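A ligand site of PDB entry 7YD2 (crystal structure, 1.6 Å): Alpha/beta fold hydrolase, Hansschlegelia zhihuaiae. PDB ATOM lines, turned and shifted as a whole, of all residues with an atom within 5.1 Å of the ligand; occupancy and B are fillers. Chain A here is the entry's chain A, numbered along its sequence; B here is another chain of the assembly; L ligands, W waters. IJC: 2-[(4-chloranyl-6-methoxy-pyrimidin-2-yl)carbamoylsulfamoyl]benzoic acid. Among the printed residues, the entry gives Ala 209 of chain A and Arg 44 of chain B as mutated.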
ATOM      1  N   GLY A  77      33.421   9.525 -22.943  1.00  0.00           N
ATOM      2  CA  GLY A  77      32.027   9.232 -22.650  1.00  0.00           C
ATOM      3  C   GLY A  77      31.100  10.410 -22.961  1.00  0.00           C
ATOM      4  O   GLY A  77      31.482  11.412 -23.562  1.00  0.00           O
ATOM      5  N   GLY A  78      29.864  10.265 -22.501  1.00  0.00           N
ATOM      6  CA  GLY A  78      28.831  11.209 -22.900  1.00  0.00           C
ATOM      7  C   GLY A  78      29.081  12.598 -22.338  1.00  0.00           C
ATOM      8  O   GLY A  78      29.349  12.765 -21.138  1.00  0.00           O
ATOM      9  N   GLY A  79      28.948  13.600 -23.195  1.00  0.00           N
ATOM     10  CA  GLY A  79      29.111  14.986 -22.780  1.00  0.00           C
ATOM     11  C   GLY A  79      30.535  15.397 -22.483  1.00  0.00           C
ATOM     12  O   GLY A  79      30.746  16.458 -21.878  1.00  0.00           O
ATOM     13  N   ASN A 141      20.656  18.556 -21.161  1.00  0.00           N
ATOM     14  CA  ASN A 141      21.967  18.623 -20.536  1.00  0.00           C
ATOM     15  C   ASN A 141      21.851  18.131 -19.102  1.00  0.00           C
ATOM     16  O   ASN A 141      20.809  18.278 -18.464  1.00  0.00           O
ATOM     17  CB  ASN A 141      22.511  20.069 -20.543  1.00  0.00           C
ATOM     18  CG  ASN A 141      24.036  20.130 -20.416  1.00  0.00           C
ATOM     19  OD1 ASN A 141      24.710  19.113 -20.285  1.00  0.00           O
ATOM     20  ND2 ASN A 141      24.564  21.340 -20.445  1.00  0.00           N
ATOM     21  N   SER A 142      22.929  17.523 -18.604  1.00  0.00           N
ATOM     22  CA  SER A 142      22.962  17.152 -17.203  1.00  0.00           C
ATOM     23  C   SER A 142      23.352  18.347 -16.340  1.00  0.00           C
ATOM     24  O   SER A 142      23.913  19.333 -16.818  1.00  0.00           O
ATOM     25  CB  SER A 142      23.934  16.006 -16.958  1.00  0.00           C
ATOM     26  OG  SER A 142      24.075  15.768 -15.554  1.00  0.00           O
ATOM     27  N   SER A 143      23.048  18.244 -15.051  1.00  0.00           N
ATOM     28  CA  SER A 143      23.473  19.217 -14.054  1.00  0.00           C
ATOM     29  C   SER A 143      24.648  18.663 -13.256  1.00  0.00           C
ATOM     30  O   SER A 143      24.990  17.475 -13.327  1.00  0.00           O
ATOM     31  CB  SER A 143      22.319  19.550 -13.105  1.00  0.00           C
ATOM     32  OG  SER A 143      21.955  18.406 -12.359  1.00  0.00           O
ATOM     33  N   GLY A 146      23.066  15.919 -11.132  1.00  0.00           N
ATOM     34  CA  GLY A 146      22.871  14.670 -11.844  1.00  0.00           C
ATOM     35  C   GLY A 146      24.190  13.963 -12.137  1.00  0.00           C
ATOM     36  O   GLY A 146      24.288  12.746 -11.985  1.00  0.00           O
ATOM     37  N   ALA A 147      25.209  14.725 -12.524  1.00  0.00           N
ATOM     38  CA  ALA A 147      26.509  14.118 -12.803  1.00  0.00           C
ATOM     39  C   ALA A 147      27.136  13.546 -11.532  1.00  0.00           C
ATOM     40  O   ALA A 147      27.799  12.502 -11.574  1.00  0.00           O
ATOM     41  CB  ALA A 147      27.450  15.137 -13.455  1.00  0.00           C
ATOM     42  N   ARG A 150      25.361  10.190 -11.084  1.00  0.00           N
ATOM     43  CA  ARG A 150      25.700   9.329 -12.214  1.00  0.00           C
ATOM     44  C   ARG A 150      27.118   8.791 -12.081  1.00  0.00           C
ATOM     45  O   ARG A 150      27.374   7.603 -12.338  1.00  0.00           O
ATOM     46  CB  ARG A 150      25.550  10.114 -13.523  1.00  0.00           C
ATOM     47  CG  ARG A 150      26.040   9.369 -14.767  1.00  0.00           C
ATOM     48  CD  ARG A 150      26.292  10.336 -15.930  1.00  0.00           C
ATOM     49  NE  ARG A 150      27.484  11.145 -15.681  1.00  0.00           N
ATOM     50  CZ  ARG A 150      27.791  12.261 -16.342  1.00  0.00           C
ATOM     51  NH1 ARG A 150      26.984  12.692 -17.301  1.00  0.00           N
ATOM     52  NH2 ARG A 150      28.889  12.928 -16.035  1.00  0.00           N
ATOM     53  N   ASP A 151      28.043   9.624 -11.638  1.00  0.00           N
ATOM     54  CA  ASP A 151      29.445   9.246 -11.599  1.00  0.00           C
ATOM     55  C   ASP A 151      29.813   8.538 -10.302  1.00  0.00           C
ATOM     56  O   ASP A 151      30.964   8.089 -10.163  1.00  0.00           O
ATOM     57  CB  ASP A 151      30.317  10.502 -11.823  1.00  0.00           C
ATOM     58  CG  ASP A 151      30.114  11.089 -13.225  1.00  0.00           C
ATOM     59  OD1 ASP A 151      29.505  10.378 -14.062  1.00  0.00           O
ATOM     60  OD2 ASP A 151      30.547  12.230 -13.495  1.00  0.00           O
ATOM     61  N   HIS A 208      34.333   4.572 -23.145  1.00  0.00           N
ATOM     62  CA  HIS A 208      33.881   5.036 -21.841  1.00  0.00           C
ATOM     63  C   HIS A 208      32.394   5.341 -21.949  1.00  0.00           C
ATOM     64  O   HIS A 208      31.992   6.106 -22.825  1.00  0.00           O
ATOM     65  CB  HIS A 208      34.644   6.293 -21.400  1.00  0.00           C
ATOM     66  CG  HIS A 208      34.129   6.908 -20.143  1.00  0.00           C
ATOM     67  ND1 HIS A 208      33.906   8.264 -20.017  1.00  0.00           N
ATOM     68  CD2 HIS A 208      33.820   6.369 -18.945  1.00  0.00           C
ATOM     69  CE1 HIS A 208      33.478   8.535 -18.800  1.00  0.00           C
ATOM     70  NE2 HIS A 208      33.404   7.393 -18.124  1.00  0.00           N
ATOM     71  N   ALA A 209      31.590   4.727 -21.079  1.00  0.00           N
ATOM     72  CA  ALA A 209      30.207   5.167 -20.903  1.00  0.00           C
ATOM     73  C   ALA A 209      29.446   5.208 -22.238  1.00  0.00           C
ATOM     74  O   ALA A 209      29.286   4.164 -22.888  1.00  0.00           O
ATOM     75  CB  ALA A 209      30.189   6.532 -20.210  1.00  0.00           C
ATOM     76  N   ALA A 210      28.993   6.393 -22.667  1.00  0.00           N
ATOM     77  CA  ALA A 210      28.204   6.489 -23.900  1.00  0.00           C
ATOM     78  C   ALA A 210      28.932   5.948 -25.129  1.00  0.00           C
ATOM     79  O   ALA A 210      28.273   5.482 -26.058  1.00  0.00           O
ATOM     80  CB  ALA A 210      27.776   7.929 -24.165  1.00  0.00           C
ATOM     81  N   ALA A 234      27.475   2.503 -21.091  1.00  0.00           N
ATOM     82  CA  ALA A 234      26.154   2.948 -20.660  1.00  0.00           C
ATOM     83  C   ALA A 234      24.999   2.185 -21.296  1.00  0.00           C
ATOM     84  O   ALA A 234      23.939   2.086 -20.681  1.00  0.00           O
ATOM     85  CB  ALA A 234      25.969   4.446 -20.946  1.00  0.00           C
ATOM     86  N   PHE A 257      18.748   1.927 -20.111  1.00  0.00           N
ATOM     87  CA  PHE A 257      18.688   2.308 -21.523  1.00  0.00           C
ATOM     88  C   PHE A 257      18.270   1.100 -22.359  1.00  0.00           C
ATOM     89  O   PHE A 257      18.796   0.001 -22.152  1.00  0.00           O
ATOM     90  CB  PHE A 257      20.040   2.819 -22.009  1.00  0.00           C
ATOM     91  CG  PHE A 257      20.403   4.193 -21.480  1.00  0.00           C
ATOM     92  CD1 PHE A 257      19.476   4.964 -20.796  1.00  0.00           C
ATOM     93  CD2 PHE A 257      21.680   4.686 -21.661  1.00  0.00           C
ATOM     94  CE1 PHE A 257      19.832   6.217 -20.303  1.00  0.00           C
ATOM     95  CE2 PHE A 257      22.033   5.930 -21.179  1.00  0.00           C
ATOM     96  CZ  PHE A 257      21.116   6.699 -20.504  1.00  0.00           C
ATOM     97  N   PHE A 293      20.404   6.415  -9.328  1.00  0.00           N
ATOM     98  CA  PHE A 293      21.501   6.078 -10.242  1.00  0.00           C
ATOM     99  C   PHE A 293      22.355   4.933  -9.733  1.00  0.00           C
ATOM    100  O   PHE A 293      22.992   4.256 -10.533  1.00  0.00           O
ATOM    101  CB  PHE A 293      22.401   7.285 -10.516  1.00  0.00           C
ATOM    102  CG  PHE A 293      22.391   7.747 -11.961  1.00  0.00           C
ATOM    103  CD1 PHE A 293      22.888   6.932 -12.987  1.00  0.00           C
ATOM    104  CD2 PHE A 293      21.927   9.012 -12.266  1.00  0.00           C
ATOM    105  CE1 PHE A 293      22.887   7.404 -14.320  1.00  0.00           C
ATOM    106  CE2 PHE A 293      21.911   9.477 -13.571  1.00  0.00           C
ATOM    107  CZ  PHE A 293      22.388   8.699 -14.587  1.00  0.00           C
ATOM    108  N   TRP A 296      20.348   2.152 -11.001  1.00  0.00           N
ATOM    109  CA  TRP A 296      20.520   2.119 -12.455  1.00  0.00           C
ATOM    110  C   TRP A 296      21.817   1.425 -12.839  1.00  0.00           C
ATOM    111  O   TRP A 296      21.845   0.613 -13.767  1.00  0.00           O
ATOM    112  CB  TRP A 296      20.482   3.543 -12.995  1.00  0.00           C
ATOM    113  CG  TRP A 296      20.459   3.675 -14.506  1.00  0.00           C
ATOM    114  CD1 TRP A 296      19.351   3.869 -15.296  1.00  0.00           C
ATOM    115  CD2 TRP A 296      21.592   3.664 -15.402  1.00  0.00           C
ATOM    116  NE1 TRP A 296      19.724   3.982 -16.620  1.00  0.00           N
ATOM    117  CE2 TRP A 296      21.092   3.857 -16.702  1.00  0.00           C
ATOM    118  CE3 TRP A 296      22.970   3.517 -15.224  1.00  0.00           C
ATOM    119  CZ2 TRP A 296      21.918   3.901 -17.837  1.00  0.00           C
ATOM    120  CZ3 TRP A 296      23.800   3.570 -16.359  1.00  0.00           C
ATOM    121  CH2 TRP A 296      23.264   3.753 -17.641  1.00  0.00           C
ATOM    122  N   TRP A 297      22.921   1.736 -12.137  1.00  0.00           N
ATOM    123  CA  TRP A 297      24.178   1.061 -12.433  1.00  0.00           C
ATOM    124  C   TRP A 297      24.131  -0.427 -12.092  1.00  0.00           C
ATOM    125  O   TRP A 297      24.755  -1.223 -12.788  1.00  0.00           O
ATOM    126  CB  TRP A 297      25.335   1.753 -11.700  1.00  0.00           C
ATOM    127  CG  TRP A 297      25.864   2.948 -12.442  1.00  0.00           C
ATOM    128  CD1 TRP A 297      25.852   4.255 -12.022  1.00  0.00           C
ATOM    129  CD2 TRP A 297      26.464   2.952 -13.745  1.00  0.00           C
ATOM    130  NE1 TRP A 297      26.410   5.064 -12.991  1.00  0.00           N
ATOM    131  CE2 TRP A 297      26.796   4.289 -14.053  1.00  0.00           C
ATOM    132  CE3 TRP A 297      26.754   1.946 -14.674  1.00  0.00           C
ATOM    133  CZ2 TRP A 297      27.407   4.653 -15.259  1.00  0.00           C
ATOM    134  CZ3 TRP A 297      27.351   2.303 -15.871  1.00  0.00           C
ATOM    135  CH2 TRP A 297      27.672   3.642 -16.150  1.00  0.00           C
ATOM    136  N   HIS A 333      32.942   6.468 -11.766  1.00  0.00           N
ATOM    137  CA  HIS A 333      32.632   6.235 -13.173  1.00  0.00           C
ATOM    138  C   HIS A 333      33.748   6.666 -14.120  1.00  0.00           C
ATOM    139  O   HIS A 333      33.685   6.356 -15.302  1.00  0.00           O
ATOM    140  CB  HIS A 333      31.321   6.970 -13.470  1.00  0.00           C
ATOM    141  CG  HIS A 333      30.808   6.826 -14.876  1.00  0.00           C
ATOM    142  ND1 HIS A 333      30.642   5.613 -15.495  1.00  0.00           N
ATOM    143  CD2 HIS A 333      30.401   7.763 -15.765  1.00  0.00           C
ATOM    144  CE1 HIS A 333      30.169   5.803 -16.723  1.00  0.00           C
ATOM    145  NE2 HIS A 333      30.007   7.107 -16.905  1.00  0.00           N
ATOM    146  N   VAL B  42      16.815  10.372 -12.646  1.00  0.00           N
ATOM    147  CA  VAL B  42      17.728  11.474 -12.844  1.00  0.00           C
ATOM    148  C   VAL B  42      17.827  11.880 -14.304  1.00  0.00           C
ATOM    149  O   VAL B  42      18.022  13.061 -14.608  1.00  0.00           O
ATOM    150  CB  VAL B  42      19.114  11.129 -12.273  1.00  0.00           C
ATOM    151  CG1 VAL B  42      20.078  12.328 -12.433  1.00  0.00           C
ATOM    152  CG2 VAL B  42      19.001  10.749 -10.793  1.00  0.00           C
ATOM    153  N   ILE B  43      17.664  10.941 -15.231  1.00  0.00           N
ATOM    154  CA  ILE B  43      17.728  11.249 -16.657  1.00  0.00           C
ATOM    155  C   ILE B  43      16.331  11.674 -17.095  1.00  0.00           C
ATOM    156  O   ILE B  43      15.473  10.841 -17.402  1.00  0.00           O
ATOM    157  CB  ILE B  43      18.254  10.083 -17.477  1.00  0.00           C
ATOM    158  CG1 ILE B  43      19.677   9.734 -17.044  1.00  0.00           C
ATOM    159  CG2 ILE B  43      18.218  10.429 -18.968  1.00  0.00           C
ATOM    160  CD1 ILE B  43      19.962   8.258 -17.101  1.00  0.00           C
ATOM    161  N   ARG B  44      16.142  12.993 -17.068  1.00  0.00           N
ATOM    162  CA  ARG B  44      14.839  13.582 -17.432  1.00  0.00           C
ATOM    163  C   ARG B  44      15.022  15.006 -17.976  1.00  0.00           C
ATOM    164  O   ARG B  44      16.048  15.614 -17.678  1.00  0.00           O
ATOM    165  CB  ARG B  44      13.855  13.515 -16.258  1.00  0.00           C
ATOM    166  CG  ARG B  44      14.256  14.299 -15.021  1.00  0.00           C
ATOM    167  CD  ARG B  44      13.124  14.145 -14.012  1.00  0.00           C
ATOM    168  NE  ARG B  44      13.371  14.822 -12.760  1.00  0.00           N
ATOM    169  CZ  ARG B  44      12.691  15.876 -12.328  1.00  0.00           C
ATOM    170  NH1 ARG B  44      11.700  16.364 -13.056  1.00  0.00           N
ATOM    171  NH2 ARG B  44      12.995  16.425 -11.178  1.00  0.00           N
ATOM    172  N   TYR B  45      14.044  15.492 -18.744  1.00  0.00           N
ATOM    173  CA  TYR B  45      14.040  16.854 -19.325  1.00  0.00           C
ATOM    174  C   TYR B  45      13.670  17.811 -18.203  1.00  0.00           C
ATOM    175  O   TYR B  45      12.458  18.036 -18.035  1.00  0.00           O
ATOM    176  CB  TYR B  45      12.940  16.905 -20.381  1.00  0.00           C
ATOM    177  CG  TYR B  45      12.723  18.164 -21.202  1.00  0.00           C
ATOM    178  CD1 TYR B  45      13.096  19.426 -20.767  1.00  0.00           C
ATOM    179  CD2 TYR B  45      12.078  18.095 -22.433  1.00  0.00           C
ATOM    180  CE1 TYR B  45      12.877  20.565 -21.513  1.00  0.00           C
ATOM    181  CE2 TYR B  45      11.845  19.219 -23.201  1.00  0.00           C
ATOM    182  CZ  TYR B  45      12.253  20.467 -22.735  1.00  0.00           C
ATOM    183  OH  TYR B  45      12.040  21.593 -23.471  1.00  0.00           O
ATOM    184  N   ASN B 123      18.283  22.296 -20.482  1.00  0.00           N
ATOM    185  CA  ASN B 123      17.090  21.544 -20.939  1.00  0.00           C
ATOM    186  C   ASN B 123      16.036  22.535 -21.448  1.00  0.00           C
ATOM    187  O   ASN B 123      15.397  23.179 -20.630  1.00  0.00           O
ATOM    188  CB  ASN B 123      16.620  20.612 -19.840  1.00  0.00           C
ATOM    189  CG  ASN B 123      17.684  19.642 -19.379  1.00  0.00           C
ATOM    190  OD1 ASN B 123      17.925  18.632 -20.020  1.00  0.00           O
ATOM    191  ND2 ASN B 123      18.319  19.944 -18.258  1.00  0.00           N
HETATM  192  O   IJC L   1      28.102   8.749 -20.905  1.00  0.00           O
HETATM  193  C   IJC L   1      27.829   8.741 -19.610  1.00  0.00           C
HETATM  194  C1  IJC L   1      26.485   8.274 -19.181  1.00  0.00           C
HETATM  195  C2  IJC L   1      26.441   7.223 -18.279  1.00  0.00           C
HETATM  196  C3  IJC L   1      25.217   6.737 -17.843  1.00  0.00           C
HETATM  197  O1  IJC L   1      28.671   9.078 -18.784  1.00  0.00           O
HETATM  198  O2  IJC L   1      25.505   9.605 -22.078  1.00  0.00           O
HETATM  199  N   IJC L   1      23.971  10.888 -20.650  1.00  0.00           N
HETATM  200  C10 IJC L   1      20.567  14.340 -16.733  1.00  0.00           C
HETATM  201  C11 IJC L   1      21.642  13.505 -16.436  1.00  0.00           C
HETATM  202  C12 IJC L   1      23.250  12.549 -14.985  1.00  0.00           C
HETATM  203  C4  IJC L   1      24.045   7.322 -18.328  1.00  0.00           C
HETATM  204  C5  IJC L   1      24.101   8.371 -19.250  1.00  0.00           C
HETATM  205  C6  IJC L   1      25.331   8.875 -19.685  1.00  0.00           C
HETATM  206  C7  IJC L   1      23.652  11.609 -19.585  1.00  0.00           C
HETATM  207  C8  IJC L   1      21.905  12.990 -18.699  1.00  0.00           C
HETATM  208  C9  IJC L   1      20.189  14.453 -18.068  1.00  0.00           C
HETATM  209  N1  IJC L   1      22.542  12.339 -19.709  1.00  0.00           N
HETATM  210  N2  IJC L   1      20.869  13.782 -19.015  1.00  0.00           N
HETATM  211  N3  IJC L   1      22.286  12.849 -17.415  1.00  0.00           N
HETATM  212  O3  IJC L   1      26.422  11.036 -20.465  1.00  0.00           O
HETATM  213  O4  IJC L   1      24.346  11.602 -18.565  1.00  0.00           O
HETATM  214  O5  IJC L   1      22.077  13.335 -15.160  1.00  0.00           O
HETATM  215  S   IJC L   1      25.362  10.111 -20.740  1.00  0.00           S
HETATM  216 CL   IJC L   1      18.824  15.493 -18.556  1.00  0.00          CL
HETATM  217  O   HOH W   1      24.991  11.932 -24.225  1.00  0.00           O
HETATM  218  O   HOH W   2      29.967  11.140 -18.661  1.00  0.00           O
HETATM  219  O   HOH W   3      24.582   7.106 -23.047  1.00  0.00           O
HETATM  220  O   HOH W   4      21.917   9.996 -22.106  1.00  0.00           O
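Water W2 lies within hydrogen-bond range of an oxygen (O1) of the ligand (2.4 Å), the backbone carbonyl oxygen (O) of Gly 78 (3.0 Å) and the guanidinium group (NH2) of Arg 150 (3.4 Å).
A ring nitrogen (NE2) of His 208 lies within hydrogen-bond range of the backbone carbonyl oxygen (O) of His 333 (3.0 Å). N of His 333 sits at hydrogen-bond distance from O of Asp 151 (3.0 Å). The indole nitrogen of Trp 297 sits at hydrogen-bond distance from the backbone carbonyl oxygen of Arg 150, 2.8 Å away. The guanidinium group (NE) of Arg 150 lies within salt-bridge range of the side-chain carboxylate (OD1) of Asp 151 (2.7 Å). OG of Ser 142 is in hydrogen-bond range of N of Ala 147, 3.4 Å away. N of Gly 146 sits at hydrogen-bond distance from OG of Ser 143, 3.0 Å away. The backbone NH (N) of Asn 141 is in hydrogen-bond range of the side-chain amide oxygen (OD1) of Asn 123 of chain B, at 3.0 Å. N of Gly 77 lies within hydrogen-bond range of ND1 of His 208 (3.2 Å).
An oxygen (O) of the ligand lies within hydrogen-bond range of the backbone NH (N) of Gly 78. An oxygen (O1) of the ligand is in hydrogen-bond range of a ring nitrogen (NE2) of His 333 (3.0 Å). N of Ala 210 sits at hydrogen-bond distance from O of the ligand (3.1 Å). NE of Arg 150 is in salt-bridge range of O1 of the ligand. The side-chain hydroxyl of Ser 142 sits at hydrogen-bond distance from an oxygen (O5) of the ligand (3.2 Å).
Gly 77 touches the ligand (C to O, 3.997 Å). Asn 141 touches the ligand. Gly 146 touches the ligand. N of Ala 147 touches C12 of the ligand, at 3.8 Å. Ala 209 touches the ligand (CB to O, 3.1 Å). Ala 234 touches the ligand (CB to C2, 3.9 Å). Phe 257 touches the ligand. Phe 293 touches the ligand. Trp 296 touches the ligand. Trp 297 touches the ligand. Val 42 of chain B touches the ligand (CG1 to O5, 3.5 Å). O of Arg 44 of chain B touches CL of the ligand, at 2.9 Å. Asn 123 of chain B touches the ligand (OD1 to CL, 3.6 Å). Hydrophobic or aromatic side chains within 4 Å of the ligand: Ala 209, Ala 210, Ala 234, Phe 257, Phe 293, Trp 296, Trp 297, His 333 and Val 42 of chain B. 18 residues have an atom within 4 Å of the ligand: Gly 77, Gly 78, Asn 141, Ser 142, Gly 146, Ala 147, Arg 150, Ala 209, Ala 210, Ala 234, Phe 257, Phe 293, Trp 296, Trp 297, His 333, Val 42 of chain B, Arg 44 of chain B and Asn 123 of chain B.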
